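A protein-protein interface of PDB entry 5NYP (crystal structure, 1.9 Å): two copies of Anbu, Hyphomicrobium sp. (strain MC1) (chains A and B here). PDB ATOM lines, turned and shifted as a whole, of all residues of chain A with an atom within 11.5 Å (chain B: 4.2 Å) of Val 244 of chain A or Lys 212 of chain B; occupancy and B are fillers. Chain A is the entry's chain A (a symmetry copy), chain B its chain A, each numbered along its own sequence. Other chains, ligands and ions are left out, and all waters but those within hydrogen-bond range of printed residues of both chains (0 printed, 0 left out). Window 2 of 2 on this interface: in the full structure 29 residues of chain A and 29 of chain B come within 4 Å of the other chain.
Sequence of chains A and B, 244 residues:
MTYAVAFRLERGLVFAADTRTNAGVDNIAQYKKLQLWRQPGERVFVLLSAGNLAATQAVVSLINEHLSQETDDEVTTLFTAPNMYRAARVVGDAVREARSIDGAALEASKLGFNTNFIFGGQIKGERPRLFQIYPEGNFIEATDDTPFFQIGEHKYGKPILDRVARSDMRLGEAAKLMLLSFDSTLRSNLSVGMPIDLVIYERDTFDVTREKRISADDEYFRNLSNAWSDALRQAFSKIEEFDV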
ATOM      1  N   PHE A 236     -33.339   1.800   7.665  1.00  0.00           N
ATOM      2  CA  PHE A 236     -31.966   1.400   7.964  1.00  0.00           C
ATOM      3  C   PHE A 236     -31.899   0.050   8.687  1.00  0.00           C
ATOM      4  O   PHE A 236     -31.022  -0.763   8.392  1.00  0.00           O
ATOM      5  CB  PHE A 236     -31.219   2.464   8.768  1.00  0.00           C
ATOM      6  CG  PHE A 236     -29.763   2.149   8.940  1.00  0.00           C
ATOM      7  CD1 PHE A 236     -28.890   2.265   7.865  1.00  0.00           C
ATOM      8  CD2 PHE A 236     -29.273   1.679  10.154  1.00  0.00           C
ATOM      9  CE1 PHE A 236     -27.549   1.948   8.003  1.00  0.00           C
ATOM     10  CE2 PHE A 236     -27.932   1.362  10.300  1.00  0.00           C
ATOM     11  CZ  PHE A 236     -27.070   1.499   9.222  1.00  0.00           C
ATOM     12  N   ILE A 239     -32.083  -2.683   5.958  1.00  0.00           N
ATOM     13  CA  ILE A 239     -30.908  -2.807   5.079  1.00  0.00           C
ATOM     14  C   ILE A 239     -29.588  -3.144   5.781  1.00  0.00           C
ATOM     15  O   ILE A 239     -28.626  -3.525   5.113  1.00  0.00           O
ATOM     16  CB  ILE A 239     -30.691  -1.556   4.183  1.00  0.00           C
ATOM     17  CG1 ILE A 239     -30.362  -0.306   5.015  1.00  0.00           C
ATOM     18  CG2 ILE A 239     -31.906  -1.328   3.291  1.00  0.00           C
ATOM     19  CD1 ILE A 239     -29.297   0.569   4.393  1.00  0.00           C
ATOM     20  N   GLU A 240     -29.528  -3.001   7.109  1.00  0.00           N
ATOM     21  CA  GLU A 240     -28.342  -3.424   7.869  1.00  0.00           C
ATOM     22  C   GLU A 240     -28.140  -4.951   7.880  1.00  0.00           C
ATOM     23  O   GLU A 240     -27.086  -5.419   8.302  1.00  0.00           O
ATOM     24  CB  GLU A 240     -28.343  -2.846   9.296  1.00  0.00           C
ATOM     25  CG  GLU A 240     -29.376  -3.424  10.251  1.00  0.00           C
ATOM     26  CD  GLU A 240     -29.489  -2.650  11.558  1.00  0.00           C
ATOM     27  OE1 GLU A 240     -28.694  -1.717  11.789  1.00  0.00           O
ATOM     28  OE2 GLU A 240     -30.383  -2.974  12.364  1.00  0.00           O
ATOM     29  N   GLU A 241     -29.141  -5.711   7.423  1.00  0.00           N
ATOM     30  CA  GLU A 241     -28.958  -7.118   7.015  1.00  0.00           C
ATOM     31  C   GLU A 241     -27.767  -7.337   6.073  1.00  0.00           C
ATOM     32  O   GLU A 241     -27.096  -8.363   6.164  1.00  0.00           O
ATOM     33  CB  GLU A 241     -30.207  -7.641   6.296  1.00  0.00           C
ATOM     34  CG  GLU A 241     -31.374  -8.000   7.198  1.00  0.00           C
ATOM     35  CD  GLU A 241     -32.559  -8.559   6.425  1.00  0.00           C
ATOM     36  OE1 GLU A 241     -32.696  -8.258   5.217  1.00  0.00           O
ATOM     37  OE2 GLU A 241     -33.360  -9.303   7.029  1.00  0.00           O
ATOM     38  N   PHE A 242     -27.534  -6.392   5.161  1.00  0.00           N
ATOM     39  CA  PHE A 242     -26.495  -6.523   4.137  1.00  0.00           C
ATOM     40  C   PHE A 242     -25.122  -6.094   4.649  1.00  0.00           C
ATOM     41  O   PHE A 242     -25.008  -5.150   5.431  1.00  0.00           O
ATOM     42  CB  PHE A 242     -26.869  -5.715   2.892  1.00  0.00           C
ATOM     43  CG  PHE A 242     -28.152  -6.166   2.243  1.00  0.00           C
ATOM     44  CD1 PHE A 242     -28.209  -7.372   1.549  1.00  0.00           C
ATOM     45  CD2 PHE A 242     -29.306  -5.391   2.326  1.00  0.00           C
ATOM     46  CE1 PHE A 242     -29.388  -7.793   0.947  1.00  0.00           C
ATOM     47  CE2 PHE A 242     -30.489  -5.809   1.728  1.00  0.00           C
ATOM     48  CZ  PHE A 242     -30.530  -7.010   1.037  1.00  0.00           C
ATOM     49  N   ASP A 243     -24.088  -6.794   4.185  1.00  0.00           N
ATOM     50  CA  ASP A 243     -22.709  -6.569   4.621  1.00  0.00           C
ATOM     51  C   ASP A 243     -21.989  -5.609   3.671  1.00  0.00           C
ATOM     52  O   ASP A 243     -22.439  -5.374   2.548  1.00  0.00           O
ATOM     53  CB  ASP A 243     -21.963  -7.913   4.684  1.00  0.00           C
ATOM     54  CG  ASP A 243     -20.812  -7.917   5.686  1.00  0.00           C
ATOM     55  OD1 ASP A 243     -20.287  -6.838   6.037  1.00  0.00           O
ATOM     56  OD2 ASP A 243     -20.424  -9.023   6.117  1.00  0.00           O
ATOM     57  N   VAL A 244     -20.878  -5.048   4.144  1.00  0.00           N
ATOM     58  CA  VAL A 244     -20.014  -4.193   3.327  1.00  0.00           C
ATOM     59  C   VAL A 244     -18.569  -4.227   3.843  1.00  0.00           C
ATOM     60  O   VAL A 244     -17.617  -3.986   3.099  1.00  0.00           O
ATOM     61  CB  VAL A 244     -20.561  -2.742   3.261  1.00  0.00           C
ATOM     62  CG1 VAL A 244     -20.432  -2.034   4.608  1.00  0.00           C
ATOM     63  CG2 VAL A 244     -19.876  -1.948   2.158  1.00  0.00           C
ATOM     64  OXT VAL A 244     -18.313  -4.511   5.015  1.00  0.00           O
ATOM     65  N   LYS B 176     -21.792   1.158   8.015  1.00  0.00           N
ATOM     66  CA  LYS B 176     -22.763   1.084   6.911  1.00  0.00           C
ATOM     67  C   LYS B 176     -23.504   2.401   6.706  1.00  0.00           C
ATOM     68  O   LYS B 176     -23.645   2.860   5.573  1.00  0.00           O
ATOM     69  CB  LYS B 176     -23.776  -0.040   7.141  1.00  0.00           C
ATOM     70  CG  LYS B 176     -23.195  -1.435   7.002  1.00  0.00           C
ATOM     71  CD  LYS B 176     -24.153  -2.490   7.526  1.00  0.00           C
ATOM     72  CE  LYS B 176     -23.438  -3.808   7.760  1.00  0.00           C
ATOM     73  NZ  LYS B 176     -24.365  -4.837   8.295  1.00  0.00           N
ATOM     74  N   LEU B 179     -21.009   4.987   5.272  1.00  0.00           N
ATOM     75  CA  LEU B 179     -20.728   4.711   3.856  1.00  0.00           C
ATOM     76  C   LEU B 179     -21.856   5.164   2.929  1.00  0.00           C
ATOM     77  O   LEU B 179     -21.592   5.646   1.828  1.00  0.00           O
ATOM     78  CB  LEU B 179     -20.427   3.220   3.633  1.00  0.00           C
ATOM     79  CG  LEU B 179     -19.062   2.727   4.117  1.00  0.00           C
ATOM     80  CD1 LEU B 179     -18.993   1.208   4.045  1.00  0.00           C
ATOM     81  CD2 LEU B 179     -17.928   3.352   3.314  1.00  0.00           C
ATOM     82  N   ILE B 196     -13.079   5.036  -0.753  1.00  0.00           N
ATOM     83  CA  ILE B 196     -13.244   5.474   0.638  1.00  0.00           C
ATOM     84  C   ILE B 196     -12.364   4.633   1.564  1.00  0.00           C
ATOM     85  O   ILE B 196     -12.440   3.405   1.538  1.00  0.00           O
ATOM     86  CB  ILE B 196     -14.718   5.354   1.099  1.00  0.00           C
ATOM     87  CG1 ILE B 196     -15.653   6.123   0.153  1.00  0.00           C
ATOM     88  CG2 ILE B 196     -14.886   5.879   2.524  1.00  0.00           C
ATOM     89  CD1 ILE B 196     -17.092   5.655   0.198  1.00  0.00           C
ATOM     90  N   ASP B 197     -11.539   5.303   2.372  1.00  0.00           N
ATOM     91  CA  ASP B 197     -10.740   4.651   3.416  1.00  0.00           C
ATOM     92  C   ASP B 197     -11.578   4.568   4.686  1.00  0.00           C
ATOM     93  O   ASP B 197     -11.976   5.600   5.220  1.00  0.00           O
ATOM     94  CB  ASP B 197      -9.457   5.443   3.715  1.00  0.00           C
ATOM     95  CG  ASP B 197      -8.468   5.443   2.556  1.00  0.00           C
ATOM     96  OD1 ASP B 197      -7.665   6.399   2.471  1.00  0.00           O
ATOM     97  OD2 ASP B 197      -8.476   4.497   1.741  1.00  0.00           O
ATOM     98  N   LEU B 198     -11.829   3.348   5.158  1.00  0.00           N
ATOM     99  CA  LEU B 198     -12.665   3.095   6.333  1.00  0.00           C
ATOM    100  C   LEU B 198     -11.822   2.460   7.432  1.00  0.00           C
ATOM    101  O   LEU B 198     -11.136   1.466   7.188  1.00  0.00           O
ATOM    102  CB  LEU B 198     -13.817   2.159   5.959  1.00  0.00           C
ATOM    103  CG  LEU B 198     -14.735   1.641   7.076  1.00  0.00           C
ATOM    104  CD1 LEU B 198     -15.488   2.783   7.741  1.00  0.00           C
ATOM    105  CD2 LEU B 198     -15.706   0.617   6.515  1.00  0.00           C
ATOM    106  N   GLU B 211      -9.105  -2.127   8.974  1.00  0.00           N
ATOM    107  CA  GLU B 211      -8.858  -1.039   8.029  1.00  0.00           C
ATOM    108  C   GLU B 211      -9.214  -1.552   6.637  1.00  0.00           C
ATOM    109  O   GLU B 211      -8.728  -2.610   6.229  1.00  0.00           O
ATOM    110  CB  GLU B 211      -7.385  -0.617   8.093  1.00  0.00           C
ATOM    111  CG  GLU B 211      -7.074   0.755   7.497  1.00  0.00           C
ATOM    112  CD  GLU B 211      -6.918   0.762   5.986  1.00  0.00           C
ATOM    113  OE1 GLU B 211      -6.291  -0.165   5.430  1.00  0.00           O
ATOM    114  OE2 GLU B 211      -7.413   1.716   5.348  1.00  0.00           O
ATOM    115  N   LYS B 212     -10.052  -0.807   5.914  1.00  0.00           N
ATOM    116  CA  LYS B 212     -10.575  -1.256   4.619  1.00  0.00           C
ATOM    117  C   LYS B 212     -10.717  -0.111   3.615  1.00  0.00           C
ATOM    118  O   LYS B 212     -11.165   0.980   3.968  1.00  0.00           O
ATOM    119  CB  LYS B 212     -11.929  -1.943   4.816  1.00  0.00           C
ATOM    120  CG  LYS B 212     -12.452  -2.646   3.573  1.00  0.00           C
ATOM    121  CD  LYS B 212     -13.573  -3.617   3.902  1.00  0.00           C
ATOM    122  CE  LYS B 212     -14.042  -4.345   2.654  1.00  0.00           C
ATOM    123  NZ  LYS B 212     -14.950  -5.480   2.974  1.00  0.00           N
ATOM    124  N   ARG B 213     -10.333  -0.382   2.367  1.00  0.00           N
ATOM    125  CA  ARG B 213     -10.502   0.548   1.254  1.00  0.00           C
ATOM    126  C   ARG B 213     -11.635   0.042   0.365  1.00  0.00           C
ATOM    127  O   ARG B 213     -11.571  -1.080  -0.139  1.00  0.00           O
ATOM    128  CB  ARG B 213      -9.204   0.656   0.454  1.00  0.00           C
ATOM    129  CG  ARG B 213      -9.225   1.722  -0.633  1.00  0.00           C
ATOM    130  CD  ARG B 213      -7.826   2.005  -1.155  1.00  0.00           C
ATOM    131  NE  ARG B 213      -6.991   2.676  -0.157  1.00  0.00           N
ATOM    132  CZ  ARG B 213      -5.690   2.938  -0.291  1.00  0.00           C
ATOM    133  NH1 ARG B 213      -5.025   2.593  -1.394  1.00  0.00           N
ATOM    134  NH2 ARG B 213      -5.042   3.556   0.694  1.00  0.00           N
ATOM    135  N   ILE B 214     -12.663   0.870   0.181  1.00  0.00           N
ATOM    136  CA  ILE B 214     -13.869   0.493  -0.561  1.00  0.00           C
ATOM    137  C   ILE B 214     -13.999   1.404  -1.779  1.00  0.00           C
ATOM    138  O   ILE B 214     -14.070   2.625  -1.633  1.00  0.00           O
ATOM    139  CB  ILE B 214     -15.134   0.621   0.322  1.00  0.00           C
ATOM    140  CG1 ILE B 214     -15.012  -0.262   1.574  1.00  0.00           C
ATOM    141  CG2 ILE B 214     -16.389   0.231  -0.458  1.00  0.00           C
ATOM    142  CD1 ILE B 214     -15.902   0.168   2.719  1.00  0.00           C
ATOM    143  N   TYR B 220     -20.443  -5.375  -2.700  1.00  0.00           N
ATOM    144  CA  TYR B 220     -21.137  -5.310  -1.410  1.00  0.00           C
ATOM    145  C   TYR B 220     -21.719  -3.911  -1.206  1.00  0.00           C
ATOM    146  O   TYR B 220     -22.884  -3.765  -0.835  1.00  0.00           O
ATOM    147  CB  TYR B 220     -20.192  -5.630  -0.243  1.00  0.00           C
ATOM    148  CG  TYR B 220     -19.818  -7.092  -0.081  1.00  0.00           C
ATOM    149  CD1 TYR B 220     -18.984  -7.736  -1.000  1.00  0.00           C
ATOM    150  CD2 TYR B 220     -20.271  -7.826   1.019  1.00  0.00           C
ATOM    151  CE1 TYR B 220     -18.634  -9.069  -0.841  1.00  0.00           C
ATOM    152  CE2 TYR B 220     -19.924  -9.158   1.187  1.00  0.00           C
ATOM    153  CZ  TYR B 220     -19.108  -9.777   0.256  1.00  0.00           C
ATOM    154  OH  TYR B 220     -18.759 -11.098   0.418  1.00  0.00           O
ATOM    155  N   PHE B 221     -20.890  -2.895  -1.451  1.00  0.00           N
ATOM    156  CA  PHE B 221     -21.288  -1.492  -1.308  1.00  0.00           C
ATOM    157  C   PHE B 221     -22.389  -1.102  -2.298  1.00  0.00           C
ATOM    158  O   PHE B 221     -23.320  -0.380  -1.935  1.00  0.00           O
ATOM    159  CB  PHE B 221     -20.066  -0.576  -1.463  1.00  0.00           C
ATOM    160  CG  PHE B 221     -20.376   0.892  -1.318  1.00  0.00           C
ATOM    161  CD1 PHE B 221     -21.022   1.372  -0.182  1.00  0.00           C
ATOM    162  CD2 PHE B 221     -20.012   1.798  -2.311  1.00  0.00           C
ATOM    163  CE1 PHE B 221     -21.309   2.724  -0.045  1.00  0.00           C
ATOM    164  CE2 PHE B 221     -20.293   3.151  -2.178  1.00  0.00           C
ATOM    165  CZ  PHE B 221     -20.943   3.615  -1.042  1.00  0.00           C
ATOM    166  N   LEU B 224     -25.563  -2.774  -1.032  1.00  0.00           N
ATOM    167  CA  LEU B 224     -26.051  -1.987   0.110  1.00  0.00           C
ATOM    168  C   LEU B 224     -26.771  -0.714  -0.345  1.00  0.00           C
ATOM    169  O   LEU B 224     -27.848  -0.398   0.162  1.00  0.00           O
ATOM    170  CB  LEU B 224     -24.895  -1.622   1.047  1.00  0.00           C
ATOM    171  CG  LEU B 224     -25.215  -0.839   2.329  1.00  0.00           C
ATOM    172  CD1 LEU B 224     -26.063  -1.663   3.284  1.00  0.00           C
ATOM    173  CD2 LEU B 224     -23.928  -0.393   3.008  1.00  0.00           C
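The backbone NH (N) of Leu 198 of chain B is in hydrogen-bond range of the backbone carbonyl oxygen (O) of Lys 212 of chain B (2.7 Å).
Of the printed residues of chain B, Glu 240 of chain A touches Lys 176.
Val 244 of chain A touches just these residues of chain B: Lys 176 (3.7 Å), Leu 179 (3.6 Å), Lys 212 (3.1 Å), Tyr 220 (3.9 Å) and Phe 221 (3.8 Å).
Ile 196 of chain B touches none of the printed residues of chain A.
No residue of chain A comes within 4 Å of Leu 198 of chain B.
Glu 211 of chain B touches none of the printed residues of chain A.
Lys 212 of chain B touches one residue of chain A.
Arg 213 of chain B touches none of the printed residues of chain A.
No residue of chain A comes within 4 Å of Ile 214 of chain B.
Tyr 220 of chain B touches two residues of chain A.
Phe 221 of chain B touches just one residue of chain A: Val 244 (3.8 Å).
Of the printed residues of chain A, Leu 224 of chain B touches Ile 239.
The nearest residue of chain A that does not touch Lys 212 of chain B is Asp 243 of chain A (6.3 Å).
The nearest printed residue of chain B that does not touch Ile 239 of chain A is Lys 176 of chain B (5.2 Å).
The side-chain amino group of Lys 176 of chain B sits at hydrogen-bond distance from the backbone carbonyl oxygen of Glu 240 of chain A.
NZ of Lys 176 of chain B lies within hydrogen-bond range of O of Phe 242 of chain A (3.0 Å).
The side-chain amino group (NZ) of Lys 212 of chain B is in salt-bridge range of the chain-end carboxylate (O) of Val 244 of chain A, 3.1 Å away.
No position is printed for both chains.
Of the 9 pairs that touch across the chains among the printed residues, none has its exchanged pair printed and touching as well.
Among the printed residues, pairs that only touch across the chains: Val 244 of chain A with Leu 179 of chain B (3.6 Å), Asp 243 of chain A with Tyr 220 of chain B (3.6 Å), Ile 239 of chain A with Leu 224 of chain B (3.7 Å), Val 244 of chain A with Lys 176 of chain B (3.7 Å), Val 244 of chain A with Phe 221 of chain B (3.8 Å) and Val 244 of chain A with Tyr 220 of chain B (3.9 Å).
Hydrophobic or aromatic side chains of chain B that line the printed part of chain A: Leu 179, Tyr 220, Phe 221 and Leu 224.
Hydrophobic or aromatic side chains of chain A within 4 Å of the printed part of chain B: Val 244.
Among the printed residues, no Asp or Glu carboxylate lies within 4 Å of a Lys or Arg side-chain nitrogen of the other chain.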
